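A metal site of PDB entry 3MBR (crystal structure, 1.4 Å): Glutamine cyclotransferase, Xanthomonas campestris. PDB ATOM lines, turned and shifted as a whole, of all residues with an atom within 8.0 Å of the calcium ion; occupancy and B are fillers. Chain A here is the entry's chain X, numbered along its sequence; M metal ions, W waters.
OE1 of Glu 156 sits at hydrogen-bond distance from N of Phe 211 (2.9 Å). The backbone carbonyl oxygen (O) of Glu 156 sits at hydrogen-bond distance from the backbone NH (N) of Leu 163, 2.8 Å away.
Of the 25 residues printed, 5 come within 4 Å of the calcium ion.
The calcium ion is bound by O of Leu 26 (2.3 Å). O of Ile 209 binds the calcium ion, at 2.3 Å. The calcium ion is bound by water W1, at 2.4 Å. The calcium ion is bound by OE2 of Glu 156 (2.4 Å). The calcium ion is bound by OE1 of Glu 154, 2.5 Å away. The calcium ion is bound by O of Leu 155.
Water W1 lies within hydrogen-bond range of the backbone carbonyl oxygen (O) of Leu 110 (2.7 Å) and the backbone carbonyl oxygen (O) of Ile 70 (2.8 Å).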
ATOM      1  N   GLU A  24      -3.426  36.631 -23.354  1.00  0.00           N
ATOM      2  CA  GLU A  24      -3.018  35.552 -22.440  1.00  0.00           C
ATOM      3  C   GLU A  24      -2.875  34.261 -23.159  1.00  0.00           C
ATOM      4  O   GLU A  24      -2.518  33.255 -22.529  1.00  0.00           O
ATOM      5  CB  GLU A  24      -4.041  35.440 -21.297  1.00  0.00           C
ATOM      6  CG  GLU A  24      -3.981  36.585 -20.307  1.00  0.00           C
ATOM      7  CD  GLU A  24      -2.697  36.788 -19.412  1.00  0.00           C
ATOM      8  OE1 GLU A  24      -1.784  36.072 -19.433  1.00  0.00           O
ATOM      9  OE2 GLU A  24      -2.652  37.802 -18.622  1.00  0.00           O
ATOM     10  N   GLY A  25      -3.159  34.175 -24.442  1.00  0.00           N
ATOM     11  CA  GLY A  25      -3.001  32.917 -25.219  1.00  0.00           C
ATOM     12  C   GLY A  25      -3.611  33.126 -26.576  1.00  0.00           C
ATOM     13  O   GLY A  25      -4.467  34.061 -26.769  1.00  0.00           O
ATOM     14  N   LEU A  26      -3.199  32.328 -27.539  1.00  0.00           N
ATOM     15  CA  LEU A  26      -3.666  32.545 -28.918  1.00  0.00           C
ATOM     16  C   LEU A  26      -3.639  31.230 -29.673  1.00  0.00           C
ATOM     17  O   LEU A  26      -2.708  30.410 -29.467  1.00  0.00           O
ATOM     18  CB  LEU A  26      -2.668  33.529 -29.605  1.00  0.00           C
ATOM     19  CG  LEU A  26      -3.069  34.111 -30.971  1.00  0.00           C
ATOM     20  CD1 LEU A  26      -4.112  35.189 -30.839  1.00  0.00           C
ATOM     21  CD2 LEU A  26      -1.788  34.682 -31.644  1.00  0.00           C
ATOM     22  N   PHE A  27      -4.634  31.016 -30.543  1.00  0.00           N
ATOM     23  CA  PHE A  27      -4.514  29.889 -31.493  1.00  0.00           C
ATOM     24  C   PHE A  27      -5.192  30.247 -32.773  1.00  0.00           C
ATOM     25  O   PHE A  27      -5.925  31.296 -32.816  1.00  0.00           O
ATOM     26  CB  PHE A  27      -4.991  28.552 -30.910  1.00  0.00           C
ATOM     27  CG  PHE A  27      -6.465  28.487 -30.599  1.00  0.00           C
ATOM     28  CD1 PHE A  27      -7.395  28.234 -31.621  1.00  0.00           C
ATOM     29  CD2 PHE A  27      -6.941  28.604 -29.278  1.00  0.00           C
ATOM     30  CE1 PHE A  27      -8.811  28.102 -31.343  1.00  0.00           C
ATOM     31  CE2 PHE A  27      -8.360  28.487 -29.024  1.00  0.00           C
ATOM     32  CZ  PHE A  27      -9.266  28.220 -30.041  1.00  0.00           C
ATOM     33  N   TYR A  28      -5.033  29.488 -33.814  1.00  0.00           N
ATOM     34  CA  TYR A  28      -5.637  29.791 -35.088  1.00  0.00           C
ATOM     35  C   TYR A  28      -6.500  28.583 -35.461  1.00  0.00           C
ATOM     36  O   TYR A  28      -6.117  27.395 -35.303  1.00  0.00           O
ATOM     37  CB  TYR A  28      -4.517  29.916 -36.133  1.00  0.00           C
ATOM     38  CG  TYR A  28      -4.988  30.069 -37.561  1.00  0.00           C
ATOM     39  CD1 TYR A  28      -5.351  28.962 -38.295  1.00  0.00           C
ATOM     40  CD2 TYR A  28      -5.143  31.296 -38.118  1.00  0.00           C
ATOM     41  CE1 TYR A  28      -5.785  29.032 -39.611  1.00  0.00           C
ATOM     42  CE2 TYR A  28      -5.564  31.404 -39.471  1.00  0.00           C
ATOM     43  CZ  TYR A  28      -5.886  30.250 -40.172  1.00  0.00           C
ATOM     44  OH  TYR A  28      -6.272  30.338 -41.509  1.00  0.00           O
ATOM     45  N   TYR A  34      -8.170  33.008 -32.249  1.00  0.00           N
ATOM     46  CA  TYR A  34      -8.909  33.030 -30.989  1.00  0.00           C
ATOM     47  C   TYR A  34      -7.874  33.493 -29.982  1.00  0.00           C
ATOM     48  O   TYR A  34      -6.724  32.980 -29.954  1.00  0.00           O
ATOM     49  CB  TYR A  34      -9.377  31.596 -30.662  1.00  0.00           C
ATOM     50  CG  TYR A  34     -10.513  31.199 -31.548  1.00  0.00           C
ATOM     51  CD1 TYR A  34     -10.251  30.725 -32.833  1.00  0.00           C
ATOM     52  CD2 TYR A  34     -11.860  31.366 -31.131  1.00  0.00           C
ATOM     53  CE1 TYR A  34     -11.262  30.360 -33.706  1.00  0.00           C
ATOM     54  CE2 TYR A  34     -12.919  30.951 -32.037  1.00  0.00           C
ATOM     55  CZ  TYR A  34     -12.605  30.471 -33.308  1.00  0.00           C
ATOM     56  OH  TYR A  34     -13.641  30.126 -34.155  1.00  0.00           O
ATOM     57  N   GLY A  69      -4.299  30.808 -20.643  1.00  0.00           N
ATOM     58  CA  GLY A  69      -4.156  30.192 -21.971  1.00  0.00           C
ATOM     59  C   GLY A  69      -5.358  29.428 -22.500  1.00  0.00           C
ATOM     60  O   GLY A  69      -6.224  28.958 -21.713  1.00  0.00           O
ATOM     61  N   ILE A  70      -5.382  29.205 -23.818  1.00  0.00           N
ATOM     62  CA  ILE A  70      -6.521  28.586 -24.515  1.00  0.00           C
ATOM     63  C   ILE A  70      -6.013  27.658 -25.598  1.00  0.00           C
ATOM     64  O   ILE A  70      -4.946  27.865 -26.163  1.00  0.00           O
ATOM     65  CB  ILE A  70      -7.449  29.653 -25.129  1.00  0.00           C
ATOM     66  CG1 ILE A  70      -6.610  30.633 -26.001  1.00  0.00           C
ATOM     67  CG2 ILE A  70      -8.266  30.406 -23.993  1.00  0.00           C
ATOM     68  CD1 ILE A  70      -7.554  31.459 -26.925  1.00  0.00           C
ATOM     69  N   VAL A  71      -6.869  26.678 -25.945  1.00  0.00           N
ATOM     70  CA  VAL A  71      -6.585  25.786 -27.052  1.00  0.00           C
ATOM     71  C   VAL A  71      -7.867  25.281 -27.651  1.00  0.00           C
ATOM     72  O   VAL A  71      -8.881  25.223 -26.938  1.00  0.00           O
ATOM     73  CB  VAL A  71      -5.734  24.571 -26.506  1.00  0.00           C
ATOM     74  CG1 VAL A  71      -6.557  23.769 -25.464  1.00  0.00           C
ATOM     75  CG2 VAL A  71      -5.190  23.708 -27.569  1.00  0.00           C
ATOM     76  N   ALA A 109      -0.500  28.332 -19.792  1.00  0.00           N
ATOM     77  CA  ALA A 109      -0.755  28.228 -21.233  1.00  0.00           C
ATOM     78  C   ALA A 109      -1.120  26.786 -21.623  1.00  0.00           C
ATOM     79  O   ALA A 109      -0.829  25.832 -20.876  1.00  0.00           O
ATOM     80  CB  ALA A 109       0.381  28.775 -22.046  1.00  0.00           C
ATOM     81  N   LEU A 110      -1.723  26.647 -22.807  1.00  0.00           N
ATOM     82  CA  LEU A 110      -2.136  25.335 -23.319  1.00  0.00           C
ATOM     83  C   LEU A 110      -1.820  25.256 -24.773  1.00  0.00           C
ATOM     84  O   LEU A 110      -1.904  26.285 -25.448  1.00  0.00           O
ATOM     85  CB  LEU A 110      -3.700  25.157 -23.238  1.00  0.00           C
ATOM     86  CG  LEU A 110      -4.288  24.883 -21.907  1.00  0.00           C
ATOM     87  CD1 LEU A 110      -5.821  24.939 -21.983  1.00  0.00           C
ATOM     88  CD2 LEU A 110      -3.830  23.467 -21.380  1.00  0.00           C
ATOM     89  N   THR A 111      -1.589  24.049 -25.299  1.00  0.00           N
ATOM     90  CA  THR A 111      -1.683  23.829 -26.724  1.00  0.00           C
ATOM     91  C   THR A 111      -2.077  22.355 -26.895  1.00  0.00           C
ATOM     92  O   THR A 111      -2.390  21.704 -25.897  1.00  0.00           O
ATOM     93  CB  THR A 111      -0.405  24.209 -27.492  1.00  0.00           C
ATOM     94  OG1 THR A 111      -0.672  24.109 -28.904  1.00  0.00           O
ATOM     95  CG2 THR A 111       0.809  23.306 -27.156  1.00  0.00           C
ATOM     96  N   SER A 112      -2.049  21.820 -28.115  1.00  0.00           N
ATOM     97  CA  SER A 112      -2.382  20.394 -28.321  1.00  0.00           C
ATOM     98  C   SER A 112      -1.705  19.897 -29.530  1.00  0.00           C
ATOM     99  O   SER A 112      -1.402  20.672 -30.483  1.00  0.00           O
ATOM    100  CB  SER A 112      -3.861  20.270 -28.418  1.00  0.00           C
ATOM    101  OG  SER A 112      -4.355  20.798 -29.647  1.00  0.00           O
ATOM    102  N   ASN A 153       5.089  31.386 -20.705  1.00  0.00           N
ATOM    103  CA  ASN A 153       3.792  32.060 -20.520  1.00  0.00           C
ATOM    104  C   ASN A 153       2.910  31.720 -21.797  1.00  0.00           C
ATOM    105  O   ASN A 153       1.703  32.127 -21.817  1.00  0.00           O
ATOM    106  CB  ASN A 153       3.882  33.639 -20.312  1.00  0.00           C
ATOM    107  CG  ASN A 153       4.280  34.400 -21.612  1.00  0.00           C
ATOM    108  OD1 ASN A 153       4.780  33.833 -22.524  1.00  0.00           O
ATOM    109  ND2 ASN A 153       4.039  35.675 -21.674  1.00  0.00           N
ATOM    110  N   GLU A 154       3.458  31.056 -22.859  1.00  0.00           N
ATOM    111  CA  GLU A 154       2.589  30.688 -23.996  1.00  0.00           C
ATOM    112  C   GLU A 154       3.169  29.509 -24.715  1.00  0.00           C
ATOM    113  O   GLU A 154       4.415  29.381 -24.800  1.00  0.00           O
ATOM    114  CB  GLU A 154       2.486  31.916 -24.938  1.00  0.00           C
ATOM    115  CG  GLU A 154       1.795  31.694 -26.306  1.00  0.00           C
ATOM    116  CD  GLU A 154       0.330  31.241 -26.336  1.00  0.00           C
ATOM    117  OE1 GLU A 154      -0.310  31.329 -27.405  1.00  0.00           O
ATOM    118  OE2 GLU A 154      -0.132  30.648 -25.299  1.00  0.00           O
ATOM    119  N   LEU A 155       2.289  28.644 -25.231  1.00  0.00           N
ATOM    120  CA  LEU A 155       2.721  27.438 -25.966  1.00  0.00           C
ATOM    121  C   LEU A 155       2.051  27.381 -27.325  1.00  0.00           C
ATOM    122  O   LEU A 155       0.913  27.946 -27.516  1.00  0.00           O
ATOM    123  CB  LEU A 155       2.206  26.193 -25.211  1.00  0.00           C
ATOM    124  CG  LEU A 155       2.826  25.976 -23.800  1.00  0.00           C
ATOM    125  CD1 LEU A 155       2.217  24.710 -23.180  1.00  0.00           C
ATOM    126  CD2 LEU A 155       4.318  25.890 -23.813  1.00  0.00           C
ATOM    127  N   GLU A 156       2.682  26.653 -28.245  1.00  0.00           N
ATOM    128  CA  GLU A 156       1.998  26.345 -29.493  1.00  0.00           C
ATOM    129  C   GLU A 156       2.670  25.104 -30.070  1.00  0.00           C
ATOM    130  O   GLU A 156       3.919  25.055 -30.181  1.00  0.00           O
ATOM    131  CB  GLU A 156       2.137  27.507 -30.465  1.00  0.00           C
ATOM    132  CG  GLU A 156       1.306  27.302 -31.755  1.00  0.00           C
ATOM    133  CD  GLU A 156      -0.189  27.247 -31.520  1.00  0.00           C
ATOM    134  OE1 GLU A 156      -0.877  27.018 -32.548  1.00  0.00           O
ATOM    135  OE2 GLU A 156      -0.695  27.514 -30.394  1.00  0.00           O
ATOM    136  N   TRP A 157       1.896  24.132 -30.515  1.00  0.00           N
ATOM    137  CA  TRP A 157       2.411  22.955 -31.158  1.00  0.00           C
ATOM    138  C   TRP A 157       2.649  23.204 -32.613  1.00  0.00           C
ATOM    139  O   TRP A 157       1.717  23.653 -33.307  1.00  0.00           O
ATOM    140  CB  TRP A 157       1.411  21.792 -31.039  1.00  0.00           C
ATOM    141  CG  TRP A 157       2.012  20.479 -31.392  1.00  0.00           C
ATOM    142  CD1 TRP A 157       1.983  19.878 -32.613  1.00  0.00           C
ATOM    143  CD2 TRP A 157       2.761  19.656 -30.534  1.00  0.00           C
ATOM    144  NE1 TRP A 157       2.675  18.654 -32.558  1.00  0.00           N
ATOM    145  CE2 TRP A 157       3.161  18.500 -31.293  1.00  0.00           C
ATOM    146  CE3 TRP A 157       3.128  19.733 -29.192  1.00  0.00           C
ATOM    147  CZ2 TRP A 157       3.844  17.429 -30.727  1.00  0.00           C
ATOM    148  CZ3 TRP A 157       3.852  18.619 -28.625  1.00  0.00           C
ATOM    149  CH2 TRP A 157       4.196  17.528 -29.411  1.00  0.00           C
ATOM    150  N   LEU A 163       6.569  24.875 -29.227  1.00  0.00           N
ATOM    151  CA  LEU A 163       7.152  26.208 -29.085  1.00  0.00           C
ATOM    152  C   LEU A 163       6.653  26.769 -27.774  1.00  0.00           C
ATOM    153  O   LEU A 163       5.453  26.671 -27.425  1.00  0.00           O
ATOM    154  CB  LEU A 163       6.699  27.152 -30.181  1.00  0.00           C
ATOM    155  CG  LEU A 163       7.178  26.860 -31.630  1.00  0.00           C
ATOM    156  CD1 LEU A 163       6.902  27.995 -32.577  1.00  0.00           C
ATOM    157  CD2 LEU A 163       8.534  26.364 -31.744  1.00  0.00           C
ATOM    158  N   ASN A 207       2.820  37.079 -25.878  1.00  0.00           N
ATOM    159  CA  ASN A 207       1.980  36.199 -25.078  1.00  0.00           C
ATOM    160  C   ASN A 207       1.051  35.410 -25.960  1.00  0.00           C
ATOM    161  O   ASN A 207       0.140  34.732 -25.451  1.00  0.00           O
ATOM    162  CB  ASN A 207       1.205  36.997 -24.019  1.00  0.00           C
ATOM    163  CG  ASN A 207       1.050  36.258 -22.776  1.00  0.00           C
ATOM    164  OD1 ASN A 207       1.237  36.907 -21.747  1.00  0.00           O
ATOM    165  ND2 ASN A 207       0.559  35.044 -22.812  1.00  0.00           N
ATOM    166  N   GLY A 208       1.202  35.446 -27.286  1.00  0.00           N
ATOM    167  CA  GLY A 208       0.302  34.707 -28.166  1.00  0.00           C
ATOM    168  C   GLY A 208       1.153  34.113 -29.281  1.00  0.00           C
ATOM    169  O   GLY A 208       1.867  34.907 -29.960  1.00  0.00           O
ATOM    170  N   ILE A 209       1.118  32.818 -29.450  1.00  0.00           N
ATOM    171  CA  ILE A 209       1.822  32.151 -30.551  1.00  0.00           C
ATOM    172  C   ILE A 209       0.769  31.249 -31.195  1.00  0.00           C
ATOM    173  O   ILE A 209       0.240  30.369 -30.483  1.00  0.00           O
ATOM    174  CB  ILE A 209       3.028  31.309 -30.074  1.00  0.00           C
ATOM    175  CG1 ILE A 209       4.029  32.196 -29.298  1.00  0.00           C
ATOM    176  CG2 ILE A 209       3.653  30.686 -31.322  1.00  0.00           C
ATOM    177  CD1 ILE A 209       5.053  31.355 -28.528  1.00  0.00           C
ATOM    178  N   ALA A 210       0.469  31.446 -32.465  1.00  0.00           N
ATOM    179  CA  ALA A 210      -0.576  30.640 -33.107  1.00  0.00           C
ATOM    180  C   ALA A 210      -0.078  30.042 -34.442  1.00  0.00           C
ATOM    181  O   ALA A 210       0.475  30.791 -35.247  1.00  0.00           O
ATOM    182  CB  ALA A 210      -1.842  31.446 -33.356  1.00  0.00           C
ATOM    183  N   PHE A 211      -0.329  28.801 -34.710  1.00  0.00           N
ATOM    184  CA  PHE A 211       0.118  28.186 -35.923  1.00  0.00           C
ATOM    185  C   PHE A 211      -1.072  27.753 -36.774  1.00  0.00           C
ATOM    186  O   PHE A 211      -2.036  27.082 -36.271  1.00  0.00           O
ATOM    187  CB  PHE A 211       0.987  26.965 -35.568  1.00  0.00           C
ATOM    188  CG  PHE A 211       1.564  26.321 -36.765  1.00  0.00           C
ATOM    189  CD1 PHE A 211       2.368  27.018 -37.644  1.00  0.00           C
ATOM    190  CD2 PHE A 211       1.321  24.959 -37.019  1.00  0.00           C
ATOM    191  CE1 PHE A 211       2.956  26.404 -38.764  1.00  0.00           C
ATOM    192  CE2 PHE A 211       1.958  24.314 -38.139  1.00  0.00           C
ATOM    193  CZ  PHE A 211       2.721  25.048 -38.998  1.00  0.00           C
ATOM    194  N   PHE A 219       2.031  32.872 -36.268  1.00  0.00           N
ATOM    195  CA  PHE A 219       1.715  34.238 -35.883  1.00  0.00           C
ATOM    196  C   PHE A 219       2.131  34.480 -34.417  1.00  0.00           C
ATOM    197  O   PHE A 219       1.956  33.609 -33.558  1.00  0.00           O
ATOM    198  CB  PHE A 219       0.183  34.414 -35.943  1.00  0.00           C
ATOM    199  CG  PHE A 219      -0.391  34.174 -37.329  1.00  0.00           C
ATOM    200  CD1 PHE A 219      -0.176  35.075 -38.375  1.00  0.00           C
ATOM    201  CD2 PHE A 219      -1.128  33.027 -37.561  1.00  0.00           C
ATOM    202  CE1 PHE A 219      -0.762  34.830 -39.629  1.00  0.00           C
ATOM    203  CE2 PHE A 219      -1.678  32.797 -38.784  1.00  0.00           C
ATOM    204  CZ  PHE A 219      -1.481  33.686 -39.819  1.00  0.00           C
HETATM  205 CA    CA M   1      -0.836  29.295 -28.741  1.00  0.00          CA
HETATM  206  O   HOH W   1      -2.472  27.958 -27.550  1.00  0.00           O
